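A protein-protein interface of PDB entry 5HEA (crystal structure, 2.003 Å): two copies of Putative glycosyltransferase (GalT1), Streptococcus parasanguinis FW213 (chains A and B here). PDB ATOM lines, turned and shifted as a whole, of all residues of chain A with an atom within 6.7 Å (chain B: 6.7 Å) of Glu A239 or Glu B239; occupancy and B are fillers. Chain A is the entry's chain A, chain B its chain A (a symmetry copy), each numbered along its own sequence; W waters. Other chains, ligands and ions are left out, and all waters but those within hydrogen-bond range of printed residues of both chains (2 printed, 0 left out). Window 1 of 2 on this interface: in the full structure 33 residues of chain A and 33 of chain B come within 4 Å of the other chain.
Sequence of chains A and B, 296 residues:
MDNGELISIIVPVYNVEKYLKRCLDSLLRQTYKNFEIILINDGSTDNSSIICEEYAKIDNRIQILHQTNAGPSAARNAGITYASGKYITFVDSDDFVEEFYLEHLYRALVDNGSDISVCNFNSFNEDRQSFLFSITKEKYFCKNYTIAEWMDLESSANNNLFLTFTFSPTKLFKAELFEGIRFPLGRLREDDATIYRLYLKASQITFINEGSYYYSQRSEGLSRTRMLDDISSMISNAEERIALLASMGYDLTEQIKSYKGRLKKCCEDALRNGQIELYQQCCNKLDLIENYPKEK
Of the 17 printed residues of chain A, 7 touch a printed residue of chain B. Printed residues of chain A that touch a printed residue of chain B: Glu A239, Glu A240, Ile A242, Ala A243, Leu A244, Tyr A259 and Lys A285. Of the 17 printed residues of chain B, 7 touch a printed residue of chain A. Hydrophobic or aromatic side chains of chain B within 4 Å of the printed part of chain A: Ile B242, Ala B243, Leu B244 and Tyr B259.
Glu A239 touches three residues of chain B. Of the printed residues of chain B, Leu A244 touches Lys B285. Of the printed residues of chain A, Ile B242 touches Ala A243. Printed residues of chain A within 4 Å of Ala B243: Glu A239 (3.7 Å), Ile A242 (3.8 Å) and Tyr A259 (3.8 Å). Of the printed residues of chain A, Leu B244 touches Lys A285. The nearest residue of chain B that does not touch Glu A239 is Ser B236 (5.2 Å). The nearest printed residue of chain A that does not touch Leu B244 is Tyr A259 (4.4 Å).
O of Glu B239 touches O of Glu A239, at 3.6 Å. OE1 of Glu A239 touches CB of Glu B240, 3.7 Å away. CB of Ala B243 touches CG of Glu A239, 3.7 Å away. Glu A240 touches Glu B239 (CB to OE1, 3.7 Å). CA of Ala B243 touches CG2 of Ile A242, at 3.8 Å. Glu B239 touches Ala A243. CE2 of Tyr B259 touches O of Ala A243, at 3.8 Å. Lys B285 touches Leu A244 (O to CD2, 3.9 Å). O of Ala B243 touches CE2 of Tyr A259, 3.8 Å away. Lys A285 touches Leu B244.
Water W1 lies within hydrogen-bond range of the side-chain carboxylate (OE1) of Glu A239 and the backbone carbonyl oxygen (O) of Ser B236. Water W2 lies within hydrogen-bond range of the side-chain carboxylate (OE1) of Glu B239 and the backbone carbonyl oxygen (O) of Ser A236.
Glu A239 touches Glu B240, and with the chains exchanged Glu A240 touches Glu B239. Glu A239 touches Ala B243, and with the chains exchanged Ala A243 touches Glu B239. Ile A242 touches Ala B243, and with the chains exchanged Ala A243 touches Ile B242. Leu A244 touches Lys B285, and with the chains exchanged Lys A285 touches Leu B244.
OE2 of Glu A239 is in salt-bridge range of NZ of Lys A285 (2.5 Å). OE2 of Glu B239 is in hydrogen-bond range of OH of Tyr B259, 2.5 Å away. The side-chain carboxylate of Glu B239 lies within salt-bridge range of the side-chain amino group of Lys B285. OE2 of Glu A239 lies within hydrogen-bond range of OH of Tyr A259, at 2.5 Å.
The side-chain amino group (NZ) of Lys B285 lies within salt-bridge range of the side-chain carboxylate (OE2) of Glu A240. NZ of Lys A285 lies within salt-bridge range of OE2 of Glu B240 (2.8 Å).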
ATOM      1  N   SER A 232     -15.108 -10.195  17.546  1.00  0.00           N
ATOM      2  CA  SER A 232     -15.164 -11.323  18.461  1.00  0.00           C
ATOM      3  C   SER A 232     -16.505 -11.446  19.181  1.00  0.00           C
ATOM      4  O   SER A 232     -17.068 -12.536  19.255  1.00  0.00           O
ATOM      5  CB  SER A 232     -14.050 -11.234  19.493  1.00  0.00           C
ATOM      6  OG  SER A 232     -14.014 -12.431  20.220  1.00  0.00           O
ATOM      7  N   SER A 233     -16.996 -10.334  19.730  1.00  0.00           N
ATOM      8  CA  SER A 233     -18.316 -10.305  20.368  1.00  0.00           C
ATOM      9  C   SER A 233     -19.471 -10.643  19.426  1.00  0.00           C
ATOM     10  O   SER A 233     -20.421 -11.335  19.811  1.00  0.00           O
ATOM     11  CB  SER A 233     -18.567  -8.932  20.974  1.00  0.00           C
ATOM     12  OG  SER A 233     -17.833  -8.819  22.171  1.00  0.00           O
ATOM     13  N   MET A 234     -19.395 -10.133  18.203  1.00  0.00           N
ATOM     14  CA  MET A 234     -20.400 -10.426  17.183  1.00  0.00           C
ATOM     15  C   MET A 234     -20.630 -11.949  17.078  1.00  0.00           C
ATOM     16  O   MET A 234     -21.768 -12.422  16.990  1.00  0.00           O
ATOM     17  CB  MET A 234     -19.952  -9.850  15.836  1.00  0.00           C
ATOM     18  CG  MET A 234     -20.973  -9.994  14.712  1.00  0.00           C
ATOM     19  SD  MET A 234     -20.381  -9.374  13.116  1.00  0.00           S
ATOM     20  CE  MET A 234     -18.934 -10.410  12.822  1.00  0.00           C
ATOM     21  N   ILE A 235     -19.540 -12.704  17.116  1.00  0.00           N
ATOM     22  CA  ILE A 235     -19.605 -14.153  16.975  1.00  0.00           C
ATOM     23  C   ILE A 235     -20.042 -14.800  18.279  1.00  0.00           C
ATOM     24  O   ILE A 235     -20.976 -15.592  18.290  1.00  0.00           O
ATOM     25  CB  ILE A 235     -18.244 -14.724  16.502  1.00  0.00           C
ATOM     26  CG1 ILE A 235     -17.885 -14.124  15.144  1.00  0.00           C
ATOM     27  CG2 ILE A 235     -18.291 -16.239  16.405  1.00  0.00           C
ATOM     28  CD1 ILE A 235     -19.004 -14.299  14.125  1.00  0.00           C
ATOM     29  N   SER A 236     -19.375 -14.467  19.386  1.00  0.00           N
ATOM     30  CA  SER A 236     -19.711 -15.110  20.662  1.00  0.00           C
ATOM     31  C   SER A 236     -21.136 -14.766  21.149  1.00  0.00           C
ATOM     32  O   SER A 236     -21.812 -15.620  21.734  1.00  0.00           O
ATOM     33  CB  SER A 236     -18.658 -14.806  21.736  1.00  0.00           C
ATOM     34  OG  SER A 236     -18.636 -13.433  22.019  1.00  0.00           O
ATOM     35  N   ASN A 237     -21.601 -13.539  20.890  1.00  0.00           N
ATOM     36  CA  ASN A 237     -22.998 -13.182  21.182  1.00  0.00           C
ATOM     37  C   ASN A 237     -23.991 -14.087  20.461  1.00  0.00           C
ATOM     38  O   ASN A 237     -24.967 -14.523  21.052  1.00  0.00           O
ATOM     39  CB  ASN A 237     -23.325 -11.722  20.818  1.00  0.00           C
ATOM     40  CG  ASN A 237     -22.669 -10.717  21.755  1.00  0.00           C
ATOM     41  OD1 ASN A 237     -22.106 -11.088  22.780  1.00  0.00           O
ATOM     42  ND2 ASN A 237     -22.757  -9.436  21.410  1.00  0.00           N
ATOM     43  N   ALA A 238     -23.764 -14.325  19.169  1.00  0.00           N
ATOM     44  CA  ALA A 238     -24.664 -15.174  18.383  1.00  0.00           C
ATOM     45  C   ALA A 238     -24.640 -16.642  18.867  1.00  0.00           C
ATOM     46  O   ALA A 238     -25.673 -17.317  18.900  1.00  0.00           O
ATOM     47  CB  ALA A 238     -24.320 -15.084  16.884  1.00  0.00           C
ATOM     48  N   GLU A 239     -23.461 -17.126  19.245  1.00  0.00           N
ATOM     49  CA  GLU A 239     -23.320 -18.496  19.770  1.00  0.00           C
ATOM     50  C   GLU A 239     -24.010 -18.667  21.119  1.00  0.00           C
ATOM     51  O   GLU A 239     -24.746 -19.617  21.339  1.00  0.00           O
ATOM     52  CB  GLU A 239     -21.839 -18.880  19.860  1.00  0.00           C
ATOM     53  CG  GLU A 239     -21.240 -19.115  18.471  1.00  0.00           C
ATOM     54  CD  GLU A 239     -19.720 -19.104  18.443  1.00  0.00           C
ATOM     55  OE1 GLU A 239     -19.100 -18.782  19.481  1.00  0.00           O
ATOM     56  OE2 GLU A 239     -19.148 -19.424  17.371  1.00  0.00           O
ATOM     57  N   GLU A 240     -23.776 -17.726  22.021  1.00  0.00           N
ATOM     58  CA  GLU A 240     -24.473 -17.699  23.307  1.00  0.00           C
ATOM     59  C   GLU A 240     -26.005 -17.674  23.126  1.00  0.00           C
ATOM     60  O   GLU A 240     -26.747 -18.414  23.787  1.00  0.00           O
ATOM     61  CB  GLU A 240     -23.981 -16.462  24.067  1.00  0.00           C
ATOM     62  CG  GLU A 240     -24.574 -16.196  25.445  1.00  0.00           C
ATOM     63  CD  GLU A 240     -23.954 -14.942  26.062  1.00  0.00           C
ATOM     64  OE1 GLU A 240     -23.924 -13.867  25.396  1.00  0.00           O
ATOM     65  OE2 GLU A 240     -23.456 -15.038  27.199  1.00  0.00           O
ATOM     66  N   ARG A 241     -26.482 -16.836  22.213  1.00  0.00           N
ATOM     67  CA  ARG A 241     -27.925 -16.700  21.992  1.00  0.00           C
ATOM     68  C   ARG A 241     -28.557 -17.975  21.405  1.00  0.00           C
ATOM     69  O   ARG A 241     -29.645 -18.402  21.829  1.00  0.00           O
ATOM     70  CB  ARG A 241     -28.225 -15.479  21.111  1.00  0.00           C
ATOM     71  CG  ARG A 241     -29.671 -15.400  20.606  1.00  0.00           C
ATOM     72  CD  ARG A 241     -29.993 -14.013  20.024  1.00  0.00           C
ATOM     73  NE  ARG A 241     -29.048 -13.548  19.008  1.00  0.00           N
ATOM     74  CZ  ARG A 241     -28.221 -12.515  19.174  1.00  0.00           C
ATOM     75  NH1 ARG A 241     -28.226 -11.845  20.319  1.00  0.00           N
ATOM     76  NH2 ARG A 241     -27.394 -12.133  18.197  1.00  0.00           N
ATOM     77  N   ILE A 242     -27.881 -18.587  20.438  1.00  0.00           N
ATOM     78  CA  ILE A 242     -28.348 -19.870  19.906  1.00  0.00           C
ATOM     79  C   ILE A 242     -28.411 -20.922  21.006  1.00  0.00           C
ATOM     80  O   ILE A 242     -29.401 -21.643  21.119  1.00  0.00           O
ATOM     81  CB  ILE A 242     -27.480 -20.362  18.722  1.00  0.00           C
ATOM     82  CG1 ILE A 242     -27.763 -19.493  17.490  1.00  0.00           C
ATOM     83  CG2 ILE A 242     -27.751 -21.861  18.428  1.00  0.00           C
ATOM     84  CD1 ILE A 242     -26.674 -19.551  16.424  1.00  0.00           C
ATOM     85  N   ALA A 243     -27.368 -20.999  21.835  1.00  0.00           N
ATOM     86  CA  ALA A 243     -27.346 -22.007  22.896  1.00  0.00           C
ATOM     87  C   ALA A 243     -28.479 -21.813  23.911  1.00  0.00           C
ATOM     88  O   ALA A 243     -29.060 -22.780  24.404  1.00  0.00           O
ATOM     89  CB  ALA A 243     -25.981 -22.016  23.613  1.00  0.00           C
ATOM     90  N   LEU A 244     -28.781 -20.560  24.233  1.00  0.00           N
ATOM     91  CA  LEU A 244     -29.854 -20.260  25.170  1.00  0.00           C
ATOM     92  C   LEU A 244     -31.212 -20.610  24.586  1.00  0.00           C
ATOM     93  O   LEU A 244     -32.004 -21.284  25.224  1.00  0.00           O
ATOM     94  CB  LEU A 244     -29.852 -18.776  25.538  1.00  0.00           C
ATOM     95  CG  LEU A 244     -29.252 -18.391  26.880  1.00  0.00           C
ATOM     96  CD1 LEU A 244     -29.524 -16.905  27.097  1.00  0.00           C
ATOM     97  CD2 LEU A 244     -29.840 -19.232  28.019  1.00  0.00           C
ATOM     98  N   TYR A 259     -26.241 -16.232  12.205  1.00  0.00           N
ATOM     99  CA  TYR A 259     -24.918 -16.719  12.610  1.00  0.00           C
ATOM    100  C   TYR A 259     -24.010 -16.983  11.406  1.00  0.00           C
ATOM    101  O   TYR A 259     -22.845 -16.589  11.402  1.00  0.00           O
ATOM    102  CB  TYR A 259     -25.085 -17.997  13.447  1.00  0.00           C
ATOM    103  CG  TYR A 259     -23.811 -18.658  13.980  1.00  0.00           C
ATOM    104  CD1 TYR A 259     -22.828 -17.925  14.626  1.00  0.00           C
ATOM    105  CD2 TYR A 259     -23.639 -20.039  13.898  1.00  0.00           C
ATOM    106  CE1 TYR A 259     -21.688 -18.552  15.141  1.00  0.00           C
ATOM    107  CE2 TYR A 259     -22.507 -20.665  14.406  1.00  0.00           C
ATOM    108  CZ  TYR A 259     -21.545 -19.919  15.033  1.00  0.00           C
ATOM    109  OH  TYR A 259     -20.428 -20.551  15.535  1.00  0.00           O
ATOM    110  N   ARG A 262     -22.785 -13.754  10.010  1.00  0.00           N
ATOM    111  CA  ARG A 262     -21.733 -13.169  10.850  1.00  0.00           C
ATOM    112  C   ARG A 262     -20.378 -13.859  10.671  1.00  0.00           C
ATOM    113  O   ARG A 262     -19.345 -13.193  10.586  1.00  0.00           O
ATOM    114  CB  ARG A 262     -22.140 -13.164  12.334  1.00  0.00           C
ATOM    115  CG  ARG A 262     -23.279 -12.200  12.623  1.00  0.00           C
ATOM    116  CD  ARG A 262     -23.749 -12.285  14.085  1.00  0.00           C
ATOM    117  NE  ARG A 262     -24.778 -11.291  14.391  1.00  0.00           N
ATOM    118  CZ  ARG A 262     -25.028 -10.802  15.608  1.00  0.00           C
ATOM    119  NH1 ARG A 262     -24.312 -11.189  16.666  1.00  0.00           N
ATOM    120  NH2 ARG A 262     -25.996  -9.913  15.770  1.00  0.00           N
ATOM    121  N   LEU A 263     -20.382 -15.188  10.610  1.00  0.00           N
ATOM    122  CA  LEU A 263     -19.160 -15.946  10.366  1.00  0.00           C
ATOM    123  C   LEU A 263     -18.467 -15.510   9.070  1.00  0.00           C
ATOM    124  O   LEU A 263     -17.243 -15.352   9.030  1.00  0.00           O
ATOM    125  CB  LEU A 263     -19.466 -17.457  10.321  1.00  0.00           C
ATOM    126  CG  LEU A 263     -19.787 -18.052  11.698  1.00  0.00           C
ATOM    127  CD1 LEU A 263     -20.296 -19.487  11.539  1.00  0.00           C
ATOM    128  CD2 LEU A 263     -18.554 -17.997  12.596  1.00  0.00           C
ATOM    129  N   LYS A 285     -15.175 -22.610  11.329  1.00  0.00           N
ATOM    130  CA  LYS A 285     -16.591 -22.750  11.614  1.00  0.00           C
ATOM    131  C   LYS A 285     -17.419 -22.643  10.333  1.00  0.00           C
ATOM    132  O   LYS A 285     -18.320 -23.450  10.097  1.00  0.00           O
ATOM    133  CB  LYS A 285     -17.042 -21.730  12.683  1.00  0.00           C
ATOM    134  CG  LYS A 285     -16.585 -22.116  14.090  1.00  0.00           C
ATOM    135  CD  LYS A 285     -17.213 -21.241  15.185  1.00  0.00           C
ATOM    136  CE  LYS A 285     -16.188 -20.306  15.811  1.00  0.00           C
ATOM    137  NZ  LYS A 285     -16.691 -19.607  17.042  1.00  0.00           N
ATOM    138  N   SER B 232     -14.882 -19.723  32.518  1.00  0.00           N
ATOM    139  CA  SER B 232     -15.366 -18.975  31.370  1.00  0.00           C
ATOM    140  C   SER B 232     -15.348 -19.786  30.076  1.00  0.00           C
ATOM    141  O   SER B 232     -16.327 -19.784  29.332  1.00  0.00           O
ATOM    142  CB  SER B 232     -14.553 -17.705  31.174  1.00  0.00           C
ATOM    143  OG  SER B 232     -15.174 -16.920  30.192  1.00  0.00           O
ATOM    144  N   SER B 233     -14.226 -20.453  29.800  1.00  0.00           N
ATOM    145  CA  SER B 233     -14.119 -21.337  28.635  1.00  0.00           C
ATOM    146  C   SER B 233     -15.101 -22.508  28.649  1.00  0.00           C
ATOM    147  O   SER B 233     -15.659 -22.880  27.611  1.00  0.00           O
ATOM    148  CB  SER B 233     -12.704 -21.889  28.535  1.00  0.00           C
ATOM    149  OG  SER B 233     -11.857 -20.887  28.024  1.00  0.00           O
ATOM    150  N   MET B 234     -15.290 -23.097  29.824  1.00  0.00           N
ATOM    151  CA  MET B 234     -16.246 -24.189  29.992  1.00  0.00           C
ATOM    152  C   MET B 234     -17.618 -23.796  29.402  1.00  0.00           C
ATOM    153  O   MET B 234     -18.271 -24.587  28.713  1.00  0.00           O
ATOM    154  CB  MET B 234     -16.375 -24.539  31.478  1.00  0.00           C
ATOM    155  CG  MET B 234     -17.264 -25.743  31.774  1.00  0.00           C
ATOM    156  SD  MET B 234     -17.456 -26.081  33.543  1.00  0.00           S
ATOM    157  CE  MET B 234     -18.206 -24.553  34.140  1.00  0.00           C
ATOM    158  N   ILE B 235     -18.028 -22.561  29.659  1.00  0.00           N
ATOM    159  CA  ILE B 235     -19.325 -22.074  29.209  1.00  0.00           C
ATOM    160  C   ILE B 235     -19.277 -21.701  27.737  1.00  0.00           C
ATOM    161  O   ILE B 235     -20.107 -22.155  26.959  1.00  0.00           O
ATOM    162  CB  ILE B 235     -19.793 -20.873  30.070  1.00  0.00           C
ATOM    163  CG1 ILE B 235     -19.923 -21.311  31.528  1.00  0.00           C
ATOM    164  CG2 ILE B 235     -21.120 -20.327  29.570  1.00  0.00           C
ATOM    165  CD1 ILE B 235     -20.803 -22.547  31.679  1.00  0.00           C
ATOM    166  N   SER B 236     -18.304 -20.876  27.341  1.00  0.00           N
ATOM    167  CA  SER B 236     -18.248 -20.431  25.944  1.00  0.00           C
ATOM    168  C   SER B 236     -17.974 -21.588  24.957  1.00  0.00           C
ATOM    169  O   SER B 236     -18.514 -21.592  23.844  1.00  0.00           O
ATOM    170  CB  SER B 236     -17.245 -19.284  25.762  1.00  0.00           C
ATOM    171  OG  SER B 236     -15.947 -19.726  26.052  1.00  0.00           O
ATOM    172  N   ASN B 237     -17.167 -22.573  25.365  1.00  0.00           N
ATOM    173  CA  ASN B 237     -16.978 -23.783  24.548  1.00  0.00           C
ATOM    174  C   ASN B 237     -18.291 -24.505  24.269  1.00  0.00           C
ATOM    175  O   ASN B 237     -18.534 -24.928  23.148  1.00  0.00           O
ATOM    176  CB  ASN B 237     -16.005 -24.786  25.193  1.00  0.00           C
ATOM    177  CG  ASN B 237     -14.559 -24.308  25.168  1.00  0.00           C
ATOM    178  OD1 ASN B 237     -14.237 -23.313  24.527  1.00  0.00           O
ATOM    179  ND2 ASN B 237     -13.681 -25.031  25.856  1.00  0.00           N
ATOM    180  N   ALA B 238     -19.114 -24.687  25.302  1.00  0.00           N
ATOM    181  CA  ALA B 238     -20.396 -25.379  25.141  1.00  0.00           C
ATOM    182  C   ALA B 238     -21.371 -24.581  24.245  1.00  0.00           C
ATOM    183  O   ALA B 238     -22.110 -25.158  23.442  1.00  0.00           O
ATOM    184  CB  ALA B 238     -21.029 -25.671  26.515  1.00  0.00           C
ATOM    185  N   GLU B 239     -21.363 -23.259  24.382  1.00  0.00           N
ATOM    186  CA  GLU B 239     -22.213 -22.390  23.549  1.00  0.00           C
ATOM    187  C   GLU B 239     -21.789 -22.407  22.084  1.00  0.00           C
ATOM    188  O   GLU B 239     -22.608 -22.554  21.189  1.00  0.00           O
ATOM    189  CB  GLU B 239     -22.213 -20.960  24.102  1.00  0.00           C
ATOM    190  CG  GLU B 239     -23.012 -20.867  25.404  1.00  0.00           C
ATOM    191  CD  GLU B 239     -22.734 -19.610  26.211  1.00  0.00           C
ATOM    192  OE1 GLU B 239     -21.816 -18.846  25.842  1.00  0.00           O
ATOM    193  OE2 GLU B 239     -23.448 -19.390  27.222  1.00  0.00           O
ATOM    194  N   GLU B 240     -20.494 -22.269  21.846  1.00  0.00           N
ATOM    195  CA  GLU B 240     -19.939 -22.396  20.498  1.00  0.00           C
ATOM    196  C   GLU B 240     -20.297 -23.754  19.859  1.00  0.00           C
ATOM    197  O   GLU B 240     -20.714 -23.833  18.695  1.00  0.00           O
ATOM    198  CB  GLU B 240     -18.421 -22.215  20.610  1.00  0.00           C
ATOM    199  CG  GLU B 240     -17.600 -22.319  19.332  1.00  0.00           C
ATOM    200  CD  GLU B 240     -16.117 -22.090  19.628  1.00  0.00           C
ATOM    201  OE1 GLU B 240     -15.555 -22.747  20.551  1.00  0.00           O
ATOM    202  OE2 GLU B 240     -15.520 -21.220  18.965  1.00  0.00           O
ATOM    203  N   ARG B 241     -20.153 -24.829  20.627  1.00  0.00           N
ATOM    204  CA  ARG B 241     -20.422 -26.172  20.105  1.00  0.00           C
ATOM    205  C   ARG B 241     -21.909 -26.392  19.773  1.00  0.00           C
ATOM    206  O   ARG B 241     -22.250 -26.974  18.728  1.00  0.00           O
ATOM    207  CB  ARG B 241     -19.909 -27.243  21.078  1.00  0.00           C
ATOM    208  CG  ARG B 241     -20.372 -28.668  20.756  1.00  0.00           C
ATOM    209  CD  ARG B 241     -19.571 -29.717  21.545  1.00  0.00           C
ATOM    210  NE  ARG B 241     -19.529 -29.486  22.990  1.00  0.00           N
ATOM    211  CZ  ARG B 241     -18.424 -29.156  23.662  1.00  0.00           C
ATOM    212  NH1 ARG B 241     -17.276 -29.019  23.013  1.00  0.00           N
ATOM    213  NH2 ARG B 241     -18.454 -28.976  24.984  1.00  0.00           N
ATOM    214  N   ILE B 242     -22.793 -25.927  20.650  1.00  0.00           N
ATOM    215  CA  ILE B 242     -24.227 -25.986  20.356  1.00  0.00           C
ATOM    216  C   ILE B 242     -24.553 -25.209  19.088  1.00  0.00           C
ATOM    217  O   ILE B 242     -25.283 -25.701  18.228  1.00  0.00           O
ATOM    218  CB  ILE B 242     -25.087 -25.488  21.544  1.00  0.00           C
ATOM    219  CG1 ILE B 242     -25.047 -26.529  22.671  1.00  0.00           C
ATOM    220  CG2 ILE B 242     -26.544 -25.208  21.088  1.00  0.00           C
ATOM    221  CD1 ILE B 242     -25.442 -25.980  24.038  1.00  0.00           C
ATOM    222  N   ALA B 243     -23.997 -24.003  18.952  1.00  0.00           N
ATOM    223  CA  ALA B 243     -24.291 -23.186  17.773  1.00  0.00           C
ATOM    224  C   ALA B 243     -23.817 -23.845  16.473  1.00  0.00           C
ATOM    225  O   ALA B 243     -24.481 -23.756  15.440  1.00  0.00           O
ATOM    226  CB  ALA B 243     -23.675 -21.780  17.917  1.00  0.00           C
ATOM    227  N   LEU B 244     -22.658 -24.494  16.522  1.00  0.00           N
ATOM    228  CA  LEU B 244     -22.124 -25.175  15.351  1.00  0.00           C
ATOM    229  C   LEU B 244     -22.971 -26.380  14.979  1.00  0.00           C
ATOM    230  O   LEU B 244     -23.354 -26.535  13.831  1.00  0.00           O
ATOM    231  CB  LEU B 244     -20.693 -25.647  15.606  1.00  0.00           C
ATOM    232  CG  LEU B 244     -19.568 -24.815  15.012  1.00  0.00           C
ATOM    233  CD1 LEU B 244     -18.263 -25.572  15.243  1.00  0.00           C
ATOM    234  CD2 LEU B 244     -19.795 -24.549  13.519  1.00  0.00           C
ATOM    235  N   TYR B 259     -24.755 -28.509  28.743  1.00  0.00           N
ATOM    236  CA  TYR B 259     -24.708 -27.055  28.932  1.00  0.00           C
ATOM    237  C   TYR B 259     -25.379 -26.625  30.239  1.00  0.00           C
ATOM    238  O   TYR B 259     -24.836 -25.812  30.985  1.00  0.00           O
ATOM    239  CB  TYR B 259     -25.378 -26.368  27.732  1.00  0.00           C
ATOM    240  CG  TYR B 259     -25.420 -24.837  27.734  1.00  0.00           C
ATOM    241  CD1 TYR B 259     -24.291 -24.080  28.005  1.00  0.00           C
ATOM    242  CD2 TYR B 259     -26.585 -24.158  27.384  1.00  0.00           C
ATOM    243  CE1 TYR B 259     -24.338 -22.682  27.964  1.00  0.00           C
ATOM    244  CE2 TYR B 259     -26.638 -22.769  27.345  1.00  0.00           C
ATOM    245  CZ  TYR B 259     -25.511 -22.042  27.624  1.00  0.00           C
ATOM    246  OH  TYR B 259     -25.574 -20.666  27.580  1.00  0.00           O
ATOM    247  N   ARG B 262     -23.167 -27.428  33.127  1.00  0.00           N
ATOM    248  CA  ARG B 262     -22.050 -26.482  33.228  1.00  0.00           C
ATOM    249  C   ARG B 262     -22.468 -25.131  33.814  1.00  0.00           C
ATOM    250  O   ARG B 262     -21.762 -24.570  34.653  1.00  0.00           O
ATOM    251  CB  ARG B 262     -21.358 -26.285  31.868  1.00  0.00           C
ATOM    252  CG  ARG B 262     -20.614 -27.529  31.407  1.00  0.00           C
ATOM    253  CD  ARG B 262     -20.020 -27.357  29.999  1.00  0.00           C
ATOM    254  NE  ARG B 262     -19.222 -28.514  29.593  1.00  0.00           N
ATOM    255  CZ  ARG B 262     -18.233 -28.481  28.696  1.00  0.00           C
ATOM    256  NH1 ARG B 262     -17.879 -27.339  28.103  1.00  0.00           N
ATOM    257  NH2 ARG B 262     -17.586 -29.596  28.395  1.00  0.00           N
ATOM    258  N   LEU B 263     -23.612 -24.612  33.376  1.00  0.00           N
ATOM    259  CA  LEU B 263     -24.145 -23.368  33.920  1.00  0.00           C
ATOM    260  C   LEU B 263     -24.318 -23.438  35.441  1.00  0.00           C
ATOM    261  O   LEU B 263     -23.979 -22.492  36.160  1.00  0.00           O
ATOM    262  CB  LEU B 263     -25.490 -23.022  33.249  1.00  0.00           C
ATOM    263  CG  LEU B 263     -25.338 -22.547  31.798  1.00  0.00           C
ATOM    264  CD1 LEU B 263     -26.716 -22.443  31.138  1.00  0.00           C
ATOM    265  CD2 LEU B 263     -24.601 -21.211  31.755  1.00  0.00           C
ATOM    266  N   LYS B 285     -28.486 -16.954  32.802  1.00  0.00           N
ATOM    267  CA  LYS B 285     -28.719 -17.979  31.802  1.00  0.00           C
ATOM    268  C   LYS B 285     -29.443 -19.181  32.409  1.00  0.00           C
ATOM    269  O   LYS B 285     -30.408 -19.690  31.835  1.00  0.00           O
ATOM    270  CB  LYS B 285     -27.400 -18.385  31.110  1.00  0.00           C
ATOM    271  CG  LYS B 285     -26.913 -17.334  30.111  1.00  0.00           C
ATOM    272  CD  LYS B 285     -25.734 -17.820  29.256  1.00  0.00           C
ATOM    273  CE  LYS B 285     -24.438 -17.117  29.637  1.00  0.00           C
ATOM    274  NZ  LYS B 285     -23.314 -17.377  28.676  1.00  0.00           N
HETATM  275  O   HOH W   1     -18.827 -18.901  22.193  1.00  0.00           O
HETATM  276  O   HOH W   2     -20.469 -17.583  23.832  1.00  0.00           O
